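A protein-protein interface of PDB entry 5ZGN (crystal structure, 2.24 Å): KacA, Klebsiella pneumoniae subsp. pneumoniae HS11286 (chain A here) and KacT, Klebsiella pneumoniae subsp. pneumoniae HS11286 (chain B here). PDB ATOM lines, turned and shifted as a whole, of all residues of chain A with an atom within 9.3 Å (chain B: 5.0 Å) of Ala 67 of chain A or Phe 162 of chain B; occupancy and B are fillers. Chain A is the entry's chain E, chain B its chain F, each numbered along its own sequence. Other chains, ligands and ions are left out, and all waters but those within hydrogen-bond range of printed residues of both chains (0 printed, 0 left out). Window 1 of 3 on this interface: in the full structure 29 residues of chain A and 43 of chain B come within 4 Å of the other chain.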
ATOM      1  N   MET A  54      -9.246  -7.977  25.651  1.00  0.00           N
ATOM      2  CA  MET A  54      -8.807  -8.608  26.886  1.00  0.00           C
ATOM      3  C   MET A  54      -7.650  -7.817  27.484  1.00  0.00           C
ATOM      4  O   MET A  54      -6.492  -8.056  27.142  1.00  0.00           O
ATOM      5  CB  MET A  54      -8.369 -10.056  26.639  1.00  0.00           C
ATOM      6  CG  MET A  54      -9.131 -10.790  25.542  1.00  0.00           C
ATOM      7  SD  MET A  54     -10.568 -11.931  26.200  1.00  0.00           S
ATOM      8  CE  MET A  54     -11.907 -10.554  26.549  1.00  0.00           C
ATOM      9  N   LEU A  56      -5.094  -7.442  29.941  1.00  0.00           N
ATOM     10  CA  LEU A  56      -4.426  -8.375  30.834  1.00  0.00           C
ATOM     11  C   LEU A  56      -3.485  -7.633  31.777  1.00  0.00           C
ATOM     12  O   LEU A  56      -2.752  -6.732  31.356  1.00  0.00           O
ATOM     13  CB  LEU A  56      -3.638  -9.419  30.035  1.00  0.00           C
ATOM     14  CG  LEU A  56      -4.338 -10.165  28.891  1.00  0.00           C
ATOM     15  CD1 LEU A  56      -3.547 -11.402  28.502  1.00  0.00           C
ATOM     16  CD2 LEU A  56      -5.767 -10.546  29.250  1.00  0.00           C
ATOM     17  N   GLN A  59       0.787 -10.341  35.375  1.00  0.00           N
ATOM     18  CA  GLN A  59       0.884 -11.765  35.683  1.00  0.00           C
ATOM     19  C   GLN A  59       0.096 -12.602  34.683  1.00  0.00           C
ATOM     20  O   GLN A  59       0.583 -13.638  34.212  1.00  0.00           O
ATOM     21  CB  GLN A  59       0.410 -12.032  37.111  1.00  0.00           C
ATOM     22  CG  GLN A  59       1.520 -12.012  38.158  1.00  0.00           C
ATOM     23  CD  GLN A  59       2.434 -13.228  38.085  1.00  0.00           C
ATOM     24  OE1 GLN A  59       2.270 -14.100  37.228  1.00  0.00           O
ATOM     25  NE2 GLN A  59       3.403 -13.291  38.992  1.00  0.00           N
ATOM     26  N   SER A  60      -1.128 -12.179  34.354  1.00  0.00           N
ATOM     27  CA  SER A  60      -1.909 -12.893  33.349  1.00  0.00           C
ATOM     28  C   SER A  60      -1.238 -12.816  31.984  1.00  0.00           C
ATOM     29  O   SER A  60      -1.219 -13.800  31.235  1.00  0.00           O
ATOM     30  CB  SER A  60      -3.326 -12.321  33.281  1.00  0.00           C
ATOM     31  OG  SER A  60      -4.085 -12.693  34.418  1.00  0.00           O
ATOM     32  N   TRP A  61      -0.683 -11.649  31.645  1.00  0.00           N
ATOM     33  CA  TRP A  61       0.051 -11.504  30.394  1.00  0.00           C
ATOM     34  C   TRP A  61       1.238 -12.457  30.340  1.00  0.00           C
ATOM     35  O   TRP A  61       1.520 -13.050  29.293  1.00  0.00           O
ATOM     36  CB  TRP A  61       0.510 -10.054  30.229  1.00  0.00           C
ATOM     37  CG  TRP A  61       1.406  -9.803  29.055  1.00  0.00           C
ATOM     38  CD1 TRP A  61       2.768  -9.883  29.031  1.00  0.00           C
ATOM     39  CD2 TRP A  61       1.005  -9.405  27.738  1.00  0.00           C
ATOM     40  NE1 TRP A  61       3.240  -9.572  27.779  1.00  0.00           N
ATOM     41  CE2 TRP A  61       2.177  -9.272  26.967  1.00  0.00           C
ATOM     42  CE3 TRP A  61      -0.231  -9.153  27.136  1.00  0.00           C
ATOM     43  CZ2 TRP A  61       2.150  -8.900  25.625  1.00  0.00           C
ATOM     44  CZ3 TRP A  61      -0.256  -8.783  25.802  1.00  0.00           C
ATOM     45  CH2 TRP A  61       0.927  -8.660  25.062  1.00  0.00           C
ATOM     46  N   SER A  62       1.937 -12.628  31.464  1.00  0.00           N
ATOM     47  CA  SER A  62       3.080 -13.533  31.491  1.00  0.00           C
ATOM     48  C   SER A  62       2.648 -14.982  31.306  1.00  0.00           C
ATOM     49  O   SER A  62       3.341 -15.761  30.641  1.00  0.00           O
ATOM     50  CB  SER A  62       3.855 -13.364  32.798  1.00  0.00           C
ATOM     51  OG  SER A  62       4.432 -12.074  32.879  1.00  0.00           O
ATOM     52  N   LEU A  63       1.506 -15.363  31.885  1.00  0.00           N
ATOM     53  CA  LEU A  63       1.009 -16.724  31.705  1.00  0.00           C
ATOM     54  C   LEU A  63       0.667 -16.995  30.246  1.00  0.00           C
ATOM     55  O   LEU A  63       0.916 -18.093  29.735  1.00  0.00           O
ATOM     56  CB  LEU A  63      -0.211 -16.963  32.596  1.00  0.00           C
ATOM     57  CG  LEU A  63       0.027 -16.930  34.106  1.00  0.00           C
ATOM     58  CD1 LEU A  63      -1.273 -17.170  34.859  1.00  0.00           C
ATOM     59  CD2 LEU A  63       1.079 -17.955  34.504  1.00  0.00           C
ATOM     60  N   VAL A  64       0.100 -16.002  29.558  1.00  0.00           N
ATOM     61  CA  VAL A  64      -0.193 -16.155  28.138  1.00  0.00           C
ATOM     62  C   VAL A  64       1.101 -16.263  27.339  1.00  0.00           C
ATOM     63  O   VAL A  64       1.217 -17.092  26.429  1.00  0.00           O
ATOM     64  CB  VAL A  64      -1.072 -14.990  27.646  1.00  0.00           C
ATOM     65  CG1 VAL A  64      -1.238 -15.046  26.135  1.00  0.00           C
ATOM     66  CG2 VAL A  64      -2.428 -15.028  28.334  1.00  0.00           C
ATOM     67  N   MET A  65       2.093 -15.442  27.672  1.00  0.00           N
ATOM     68  CA  MET A  65       3.377 -15.484  26.981  1.00  0.00           C
ATOM     69  C   MET A  65       4.091 -16.815  27.219  1.00  0.00           C
ATOM     70  O   MET A  65       4.751 -17.335  26.319  1.00  0.00           O
ATOM     71  CB  MET A  65       4.265 -14.318  27.421  1.00  0.00           C
ATOM     72  CG  MET A  65       3.718 -12.947  27.043  1.00  0.00           C
ATOM     73  SD  MET A  65       3.494 -12.709  25.118  1.00  0.00           S
ATOM     74  CE  MET A  65       5.362 -12.886  24.576  1.00  0.00           C
ATOM     75  N   GLU A  66       3.949 -17.366  28.427  1.00  0.00           N
ATOM     76  CA  GLU A  66       4.532 -18.675  28.705  1.00  0.00           C
ATOM     77  C   GLU A  66       3.843 -19.762  27.888  1.00  0.00           C
ATOM     78  O   GLU A  66       4.502 -20.673  27.374  1.00  0.00           O
ATOM     79  CB  GLU A  66       4.445 -18.991  30.198  1.00  0.00           C
ATOM     80  CG  GLU A  66       5.389 -18.176  31.067  1.00  0.00           C
ATOM     81  CD  GLU A  66       5.168 -18.410  32.550  1.00  0.00           C
ATOM     82  OE1 GLU A  66       5.202 -17.427  33.321  1.00  0.00           O
ATOM     83  OE2 GLU A  66       4.951 -19.577  32.943  1.00  0.00           O
ATOM     84  N   ALA A  67       2.517 -19.682  27.764  1.00  0.00           N
ATOM     85  CA  ALA A  67       1.789 -20.646  26.946  1.00  0.00           C
ATOM     86  C   ALA A  67       2.146 -20.518  25.471  1.00  0.00           C
ATOM     87  O   ALA A  67       2.137 -21.518  24.746  1.00  0.00           O
ATOM     88  CB  ALA A  67       0.284 -20.470  27.143  1.00  0.00           C
ATOM     89  N   ILE A  68       2.461 -19.308  25.009  1.00  0.00           N
ATOM     90  CA  ILE A  68       2.788 -19.111  23.601  1.00  0.00           C
ATOM     91  C   ILE A  68       4.202 -19.593  23.300  1.00  0.00           C
ATOM     92  O   ILE A  68       4.429 -20.333  22.336  1.00  0.00           O
ATOM     93  CB  ILE A  68       2.599 -17.632  23.213  1.00  0.00           C
ATOM     94  CG1 ILE A  68       1.114 -17.266  23.211  1.00  0.00           C
ATOM     95  CG2 ILE A  68       3.221 -17.348  21.852  1.00  0.00           C
ATOM     96  CD1 ILE A  68       0.854 -15.780  23.070  1.00  0.00           C
ATOM     97  N   THR A  69       5.173 -19.184  24.121  1.00  0.00           N
ATOM     98  CA  THR A  69       6.565 -19.541  23.870  1.00  0.00           C
ATOM     99  C   THR A  69       6.875 -20.984  24.255  1.00  0.00           C
ATOM    100  O   THR A  69       7.704 -21.628  23.600  1.00  0.00           O
ATOM    101  CB  THR A  69       7.495 -18.584  24.617  1.00  0.00           C
ATOM    102  OG1 THR A  69       7.319 -18.746  26.031  1.00  0.00           O
ATOM    103  CG2 THR A  69       7.199 -17.141  24.234  1.00  0.00           C
ATOM    104  N   GLN A  70       6.229 -21.509  25.299  1.00  0.00           N
ATOM    105  CA  GLN A  70       6.421 -22.886  25.757  1.00  0.00           C
ATOM    106  C   GLN A  70       5.066 -23.587  25.757  1.00  0.00           C
ATOM    107  O   GLN A  70       4.462 -23.792  26.821  1.00  0.00           O
ATOM    108  CB  GLN A  70       7.061 -22.931  27.144  1.00  0.00           C
ATOM    109  CG  GLN A  70       7.940 -21.735  27.477  1.00  0.00           C
ATOM    110  CD  GLN A  70       9.289 -21.795  26.787  1.00  0.00           C
ATOM    111  OE1 GLN A  70       9.743 -22.865  26.379  1.00  0.00           O
ATOM    112  NE2 GLN A  70       9.941 -20.645  26.657  1.00  0.00           N
ATOM    113  N   PRO A  71       4.561 -23.971  24.588  1.00  0.00           N
ATOM    114  CA  PRO A  71       3.208 -24.537  24.509  1.00  0.00           C
ATOM    115  C   PRO A  71       3.156 -25.936  25.093  1.00  0.00           C
ATOM    116  O   PRO A  71       4.005 -26.785  24.782  1.00  0.00           O
ATOM    117  CB  PRO A  71       2.921 -24.550  23.001  1.00  0.00           C
ATOM    118  CG  PRO A  71       4.265 -24.642  22.369  1.00  0.00           C
ATOM    119  CD  PRO A  71       5.201 -23.877  23.264  1.00  0.00           C
ATOM    120  N   PRO A  72       2.179 -26.214  25.953  1.00  0.00           N
ATOM    121  CA  PRO A  72       2.014 -27.575  26.472  1.00  0.00           C
ATOM    122  C   PRO A  72       1.515 -28.530  25.398  1.00  0.00           C
ATOM    123  O   PRO A  72       0.884 -28.139  24.414  1.00  0.00           O
ATOM    124  CB  PRO A  72       0.974 -27.411  27.586  1.00  0.00           C
ATOM    125  CG  PRO A  72       0.247 -26.149  27.250  1.00  0.00           C
ATOM    126  CD  PRO A  72       1.243 -25.260  26.572  1.00  0.00           C
ATOM    127  N   ALA A  73       1.815 -29.810  25.604  1.00  0.00           N
ATOM    128  CA  ALA A  73       1.221 -30.849  24.775  1.00  0.00           C
ATOM    129  C   ALA A  73      -0.193 -31.161  25.264  1.00  0.00           C
ATOM    130  O   ALA A  73      -0.430 -31.220  26.474  1.00  0.00           O
ATOM    131  CB  ALA A  73       2.074 -32.113  24.802  1.00  0.00           C
ATOM    132  N   PHE B  70      -5.851  -9.503  22.954  1.00  0.00           N
ATOM    133  CA  PHE B  70      -5.404  -9.329  24.327  1.00  0.00           C
ATOM    134  C   PHE B  70      -4.257  -8.330  24.357  1.00  0.00           C
ATOM    135  O   PHE B  70      -3.388  -8.340  23.480  1.00  0.00           O
ATOM    136  CB  PHE B  70      -4.985 -10.669  24.961  1.00  0.00           C
ATOM    137  CG  PHE B  70      -3.921 -11.419  24.197  1.00  0.00           C
ATOM    138  CD1 PHE B  70      -4.238 -12.139  23.054  1.00  0.00           C
ATOM    139  CD2 PHE B  70      -2.610 -11.433  24.645  1.00  0.00           C
ATOM    140  CE1 PHE B  70      -3.264 -12.841  22.363  1.00  0.00           C
ATOM    141  CE2 PHE B  70      -1.632 -12.130  23.957  1.00  0.00           C
ATOM    142  CZ  PHE B  70      -1.961 -12.838  22.816  1.00  0.00           C
ATOM    143  N   TYR B 130      -3.010 -15.966  18.162  1.00  0.00           N
ATOM    144  CA  TYR B 130      -2.083 -16.526  19.136  1.00  0.00           C
ATOM    145  C   TYR B 130      -2.719 -17.545  20.072  1.00  0.00           C
ATOM    146  O   TYR B 130      -1.987 -18.265  20.758  1.00  0.00           O
ATOM    147  CB  TYR B 130      -1.448 -15.408  19.968  1.00  0.00           C
ATOM    148  CG  TYR B 130      -0.372 -14.642  19.235  1.00  0.00           C
ATOM    149  CD1 TYR B 130       0.895 -15.184  19.061  1.00  0.00           C
ATOM    150  CD2 TYR B 130      -0.622 -13.377  18.721  1.00  0.00           C
ATOM    151  CE1 TYR B 130       1.883 -14.490  18.391  1.00  0.00           C
ATOM    152  CE2 TYR B 130       0.361 -12.674  18.050  1.00  0.00           C
ATOM    153  CZ  TYR B 130       1.609 -13.234  17.888  1.00  0.00           C
ATOM    154  OH  TYR B 130       2.590 -12.537  17.223  1.00  0.00           O
ATOM    155  N   GLY B 131      -4.042 -17.625  20.131  1.00  0.00           N
ATOM    156  CA  GLY B 131      -4.665 -18.613  20.987  1.00  0.00           C
ATOM    157  C   GLY B 131      -6.154 -18.373  21.126  1.00  0.00           C
ATOM    158  O   GLY B 131      -6.741 -17.532  20.443  1.00  0.00           O
ATOM    159  N   LEU B 132      -6.745 -19.134  22.046  1.00  0.00           N
ATOM    160  CA  LEU B 132      -8.186 -19.175  22.255  1.00  0.00           C
ATOM    161  C   LEU B 132      -8.487 -18.804  23.699  1.00  0.00           C
ATOM    162  O   LEU B 132      -8.000 -19.462  24.625  1.00  0.00           O
ATOM    163  CB  LEU B 132      -8.740 -20.564  21.926  1.00  0.00           C
ATOM    164  CG  LEU B 132     -10.176 -20.878  22.350  1.00  0.00           C
ATOM    165  CD1 LEU B 132     -11.164 -19.952  21.657  1.00  0.00           C
ATOM    166  CD2 LEU B 132     -10.504 -22.337  22.066  1.00  0.00           C
ATOM    167  N   PHE B 133      -9.281 -17.755  23.888  1.00  0.00           N
ATOM    168  CA  PHE B 133      -9.737 -17.345  25.206  1.00  0.00           C
ATOM    169  C   PHE B 133     -11.152 -17.850  25.456  1.00  0.00           C
ATOM    170  O   PHE B 133     -11.947 -18.017  24.529  1.00  0.00           O
ATOM    171  CB  PHE B 133      -9.702 -15.822  25.356  1.00  0.00           C
ATOM    172  CG  PHE B 133      -8.320 -15.256  25.496  1.00  0.00           C
ATOM    173  CD1 PHE B 133      -7.707 -15.189  26.736  1.00  0.00           C
ATOM    174  CD2 PHE B 133      -7.635 -14.785  24.389  1.00  0.00           C
ATOM    175  CE1 PHE B 133      -6.433 -14.666  26.868  1.00  0.00           C
ATOM    176  CE2 PHE B 133      -6.362 -14.262  24.515  1.00  0.00           C
ATOM    177  CZ  PHE B 133      -5.761 -14.202  25.756  1.00  0.00           C
ATOM    178  N   GLY B 149      -7.140 -28.683  29.549  1.00  0.00           N
ATOM    179  CA  GLY B 149      -5.817 -28.119  29.369  1.00  0.00           C
ATOM    180  C   GLY B 149      -5.758 -26.608  29.317  1.00  0.00           C
ATOM    181  O   GLY B 149      -4.666 -26.059  29.127  1.00  0.00           O
ATOM    182  N   PHE B 150      -6.885 -25.916  29.476  1.00  0.00           N
ATOM    183  CA  PHE B 150      -6.876 -24.460  29.470  1.00  0.00           C
ATOM    184  C   PHE B 150      -6.115 -23.921  30.676  1.00  0.00           C
ATOM    185  O   PHE B 150      -6.137 -24.499  31.766  1.00  0.00           O
ATOM    186  CB  PHE B 150      -8.304 -23.913  29.469  1.00  0.00           C
ATOM    187  CG  PHE B 150      -8.973 -23.955  28.124  1.00  0.00           C
ATOM    188  CD1 PHE B 150      -9.558 -25.121  27.660  1.00  0.00           C
ATOM    189  CD2 PHE B 150      -9.019 -22.824  27.326  1.00  0.00           C
ATOM    190  CE1 PHE B 150     -10.176 -25.159  26.424  1.00  0.00           C
ATOM    191  CE2 PHE B 150      -9.634 -22.856  26.088  1.00  0.00           C
ATOM    192  CZ  PHE B 150     -10.213 -24.024  25.637  1.00  0.00           C
ATOM    193  N   ILE B 151      -5.435 -22.798  30.468  1.00  0.00           N
ATOM    194  CA  ILE B 151      -4.655 -22.140  31.510  1.00  0.00           C
ATOM    195  C   ILE B 151      -5.466 -20.970  32.049  1.00  0.00           C
ATOM    196  O   ILE B 151      -5.836 -20.061  31.296  1.00  0.00           O
ATOM    197  CB  ILE B 151      -3.293 -21.673  30.975  1.00  0.00           C
ATOM    198  CG1 ILE B 151      -2.413 -22.879  30.644  1.00  0.00           C
ATOM    199  CG2 ILE B 151      -2.609 -20.759  31.981  1.00  0.00           C
ATOM    200  CD1 ILE B 151      -1.348 -22.594  29.611  1.00  0.00           C
ATOM    201  N   GLN B 152      -5.741 -20.987  33.351  1.00  0.00           N
ATOM    202  CA  GLN B 152      -6.508 -19.917  33.974  1.00  0.00           C
ATOM    203  C   GLN B 152      -5.611 -18.728  34.291  1.00  0.00           C
ATOM    204  O   GLN B 152      -4.489 -18.888  34.781  1.00  0.00           O
ATOM    205  CB  GLN B 152      -7.187 -20.412  35.251  1.00  0.00           C
ATOM    206  CG  GLN B 152      -8.202 -19.432  35.819  1.00  0.00           C
ATOM    207  CD  GLN B 152      -8.508 -19.686  37.280  1.00  0.00           C
ATOM    208  OE1 GLN B 152      -8.261 -20.775  37.797  1.00  0.00           O
ATOM    209  NE2 GLN B 152      -9.048 -18.678  37.955  1.00  0.00           N
ATOM    210  N   LEU B 153      -6.117 -17.530  34.017  1.00  0.00           N
ATOM    211  CA  LEU B 153      -5.389 -16.304  34.301  1.00  0.00           C
ATOM    212  C   LEU B 153      -5.751 -15.810  35.702  1.00  0.00           C
ATOM    213  O   LEU B 153      -6.557 -16.416  36.410  1.00  0.00           O
ATOM    214  CB  LEU B 153      -5.668 -15.264  33.217  1.00  0.00           C
ATOM    215  CG  LEU B 153      -5.474 -15.770  31.781  1.00  0.00           C
ATOM    216  CD1 LEU B 153      -5.529 -14.622  30.786  1.00  0.00           C
ATOM    217  CD2 LEU B 153      -4.164 -16.539  31.635  1.00  0.00           C
ATOM    218  N   LEU B 160     -10.937 -15.893  33.020  1.00  0.00           N
ATOM    219  CA  LEU B 160     -10.559 -16.135  31.638  1.00  0.00           C
ATOM    220  C   LEU B 160      -9.571 -17.287  31.596  1.00  0.00           C
ATOM    221  O   LEU B 160      -8.657 -17.364  32.423  1.00  0.00           O
ATOM    222  CB  LEU B 160      -9.939 -14.884  30.990  1.00  0.00           C
ATOM    223  CG  LEU B 160     -10.842 -13.675  30.723  1.00  0.00           C
ATOM    224  CD1 LEU B 160     -10.100 -12.613  29.925  1.00  0.00           C
ATOM    225  CD2 LEU B 160     -12.117 -14.082  30.009  1.00  0.00           C
ATOM    226  N   LEU B 161      -9.755 -18.181  30.634  1.00  0.00           N
ATOM    227  CA  LEU B 161      -8.825 -19.272  30.400  1.00  0.00           C
ATOM    228  C   LEU B 161      -8.310 -19.184  28.972  1.00  0.00           C
ATOM    229  O   LEU B 161      -9.004 -18.700  28.072  1.00  0.00           O
ATOM    230  CB  LEU B 161      -9.479 -20.634  30.656  1.00  0.00           C
ATOM    231  CG  LEU B 161     -10.070 -20.802  32.057  1.00  0.00           C
ATOM    232  CD1 LEU B 161     -11.584 -20.888  31.990  1.00  0.00           C
ATOM    233  CD2 LEU B 161      -9.489 -22.023  32.748  1.00  0.00           C
ATOM    234  N   PHE B 162      -7.082 -19.651  28.773  1.00  0.00           N
ATOM    235  CA  PHE B 162      -6.374 -19.466  27.516  1.00  0.00           C
ATOM    236  C   PHE B 162      -5.729 -20.771  27.084  1.00  0.00           C
ATOM    237  O   PHE B 162      -5.202 -21.521  27.912  1.00  0.00           O
ATOM    238  CB  PHE B 162      -5.307 -18.370  27.647  1.00  0.00           C
ATOM    239  CG  PHE B 162      -4.439 -18.215  26.432  1.00  0.00           C
ATOM    240  CD1 PHE B 162      -4.898 -17.529  25.320  1.00  0.00           C
ATOM    241  CD2 PHE B 162      -3.163 -18.755  26.403  1.00  0.00           C
ATOM    242  CE1 PHE B 162      -4.100 -17.383  24.203  1.00  0.00           C
ATOM    243  CE2 PHE B 162      -2.362 -18.613  25.287  1.00  0.00           C
ATOM    244  CZ  PHE B 162      -2.831 -17.926  24.186  1.00  0.00           C
ATOM    245  N   TYR B 163      -5.778 -21.038  25.781  1.00  0.00           N
ATOM    246  CA  TYR B 163      -5.110 -22.189  25.186  1.00  0.00           C
ATOM    247  C   TYR B 163      -4.386 -21.700  23.937  1.00  0.00           C
ATOM    248  O   TYR B 163      -5.033 -21.132  23.034  1.00  0.00           O
ATOM    249  CB  TYR B 163      -6.103 -23.305  24.855  1.00  0.00           C
ATOM    250  CG  TYR B 163      -5.462 -24.668  24.725  1.00  0.00           C
ATOM    251  CD1 TYR B 163      -4.913 -25.306  25.830  1.00  0.00           C
ATOM    252  CD2 TYR B 163      -5.411 -25.319  23.501  1.00  0.00           C
ATOM    253  CE1 TYR B 163      -4.325 -26.556  25.718  1.00  0.00           C
ATOM    254  CE2 TYR B 163      -4.829 -26.568  23.379  1.00  0.00           C
ATOM    255  CZ  TYR B 163      -4.287 -27.181  24.491  1.00  0.00           C
ATOM    256  OH  TYR B 163      -3.705 -28.422  24.371  1.00  0.00           O
ATOM    257  N   PRO B 164      -3.077 -21.891  23.836  1.00  0.00           N
ATOM    258  CA  PRO B 164      -2.322 -21.304  22.725  1.00  0.00           C
ATOM    259  C   PRO B 164      -2.534 -22.054  21.416  1.00  0.00           C
ATOM    260  O   PRO B 164      -2.912 -23.227  21.382  1.00  0.00           O
ATOM    261  CB  PRO B 164      -0.868 -21.420  23.193  1.00  0.00           C
ATOM    262  CG  PRO B 164      -0.870 -22.620  24.078  1.00  0.00           C
ATOM    263  CD  PRO B 164      -2.206 -22.621  24.774  1.00  0.00           C
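N of Leu 153 of chain B is in hydrogen-bond range of O of Leu 160 of chain B, at 3.0 Å. O of Ile 151 of chain B sits at hydrogen-bond distance from N of Phe 162 of chain B.
Among the printed residues, merely in contact across the chains: Met 54 of chain A with Phe 70 of chain B (3.3 Å), Met 54 of chain A with Leu 160 of chain B (3.8 Å), Leu 56 of chain A with Phe 70 of chain B (3.9 Å), Ser 60 of chain A with Leu 153 of chain B (3.2 Å), Trp 61 of chain A with Phe 70 of chain B (3.7 Å), Leu 63 of chain A with Gln 152 of chain B (3.6 Å), Val 64 of chain A with Phe 70 of chain B (3.7 Å), Val 64 of chain A with Leu 153 of chain B (3.97 Å), Val 64 of chain A with Phe 162 of chain B (3.8 Å), Ala 67 of chain A with Ile 151 of chain B (3.6 Å), Ala 67 of chain A with Phe 162 of chain B (3.7 Å), Ala 67 of chain A with Pro 164 of chain B (3.3 Å) and Ile 68 of chain A with Tyr 130 of chain B (3.9 Å).
Of the printed residues of chain B, Leu 56 of chain A touches Phe 70 (3.9 Å). Met 65 of chain A touches none of the printed residues of chain B. Ala 67 of chain A touches three residues of chain B. No residue of chain A comes within 4 Å of Gly 131 of chain B. Ile 151 of chain B touches just one residue of chain A: Ala 67 (3.6 Å). Of the printed residues of chain A, Leu 160 of chain B touches Met 54 (3.8 Å). Phe 162 of chain B touches two residues of chain A. Printed residues of chain A within 4 Å of Pro 164 of chain B: Ala 67. The nearest printed residue of chain A that does not touch Gln 152 of chain B is Ser 60 of chain A (6.2 Å).
Printed residues of chain A that touch a printed residue of chain B: Met 54, Leu 56, Ser 60, Trp 61, Leu 63, Val 64, Ala 67 and Ile 68. Hydrophobic or aromatic side chains of chain B that line the printed part of chain A: Phe 70, Tyr 130, Ile 151, Leu 153, Leu 160, Phe 162 and Pro 164. Among the printed residues, 13 pairs touch across the chains.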
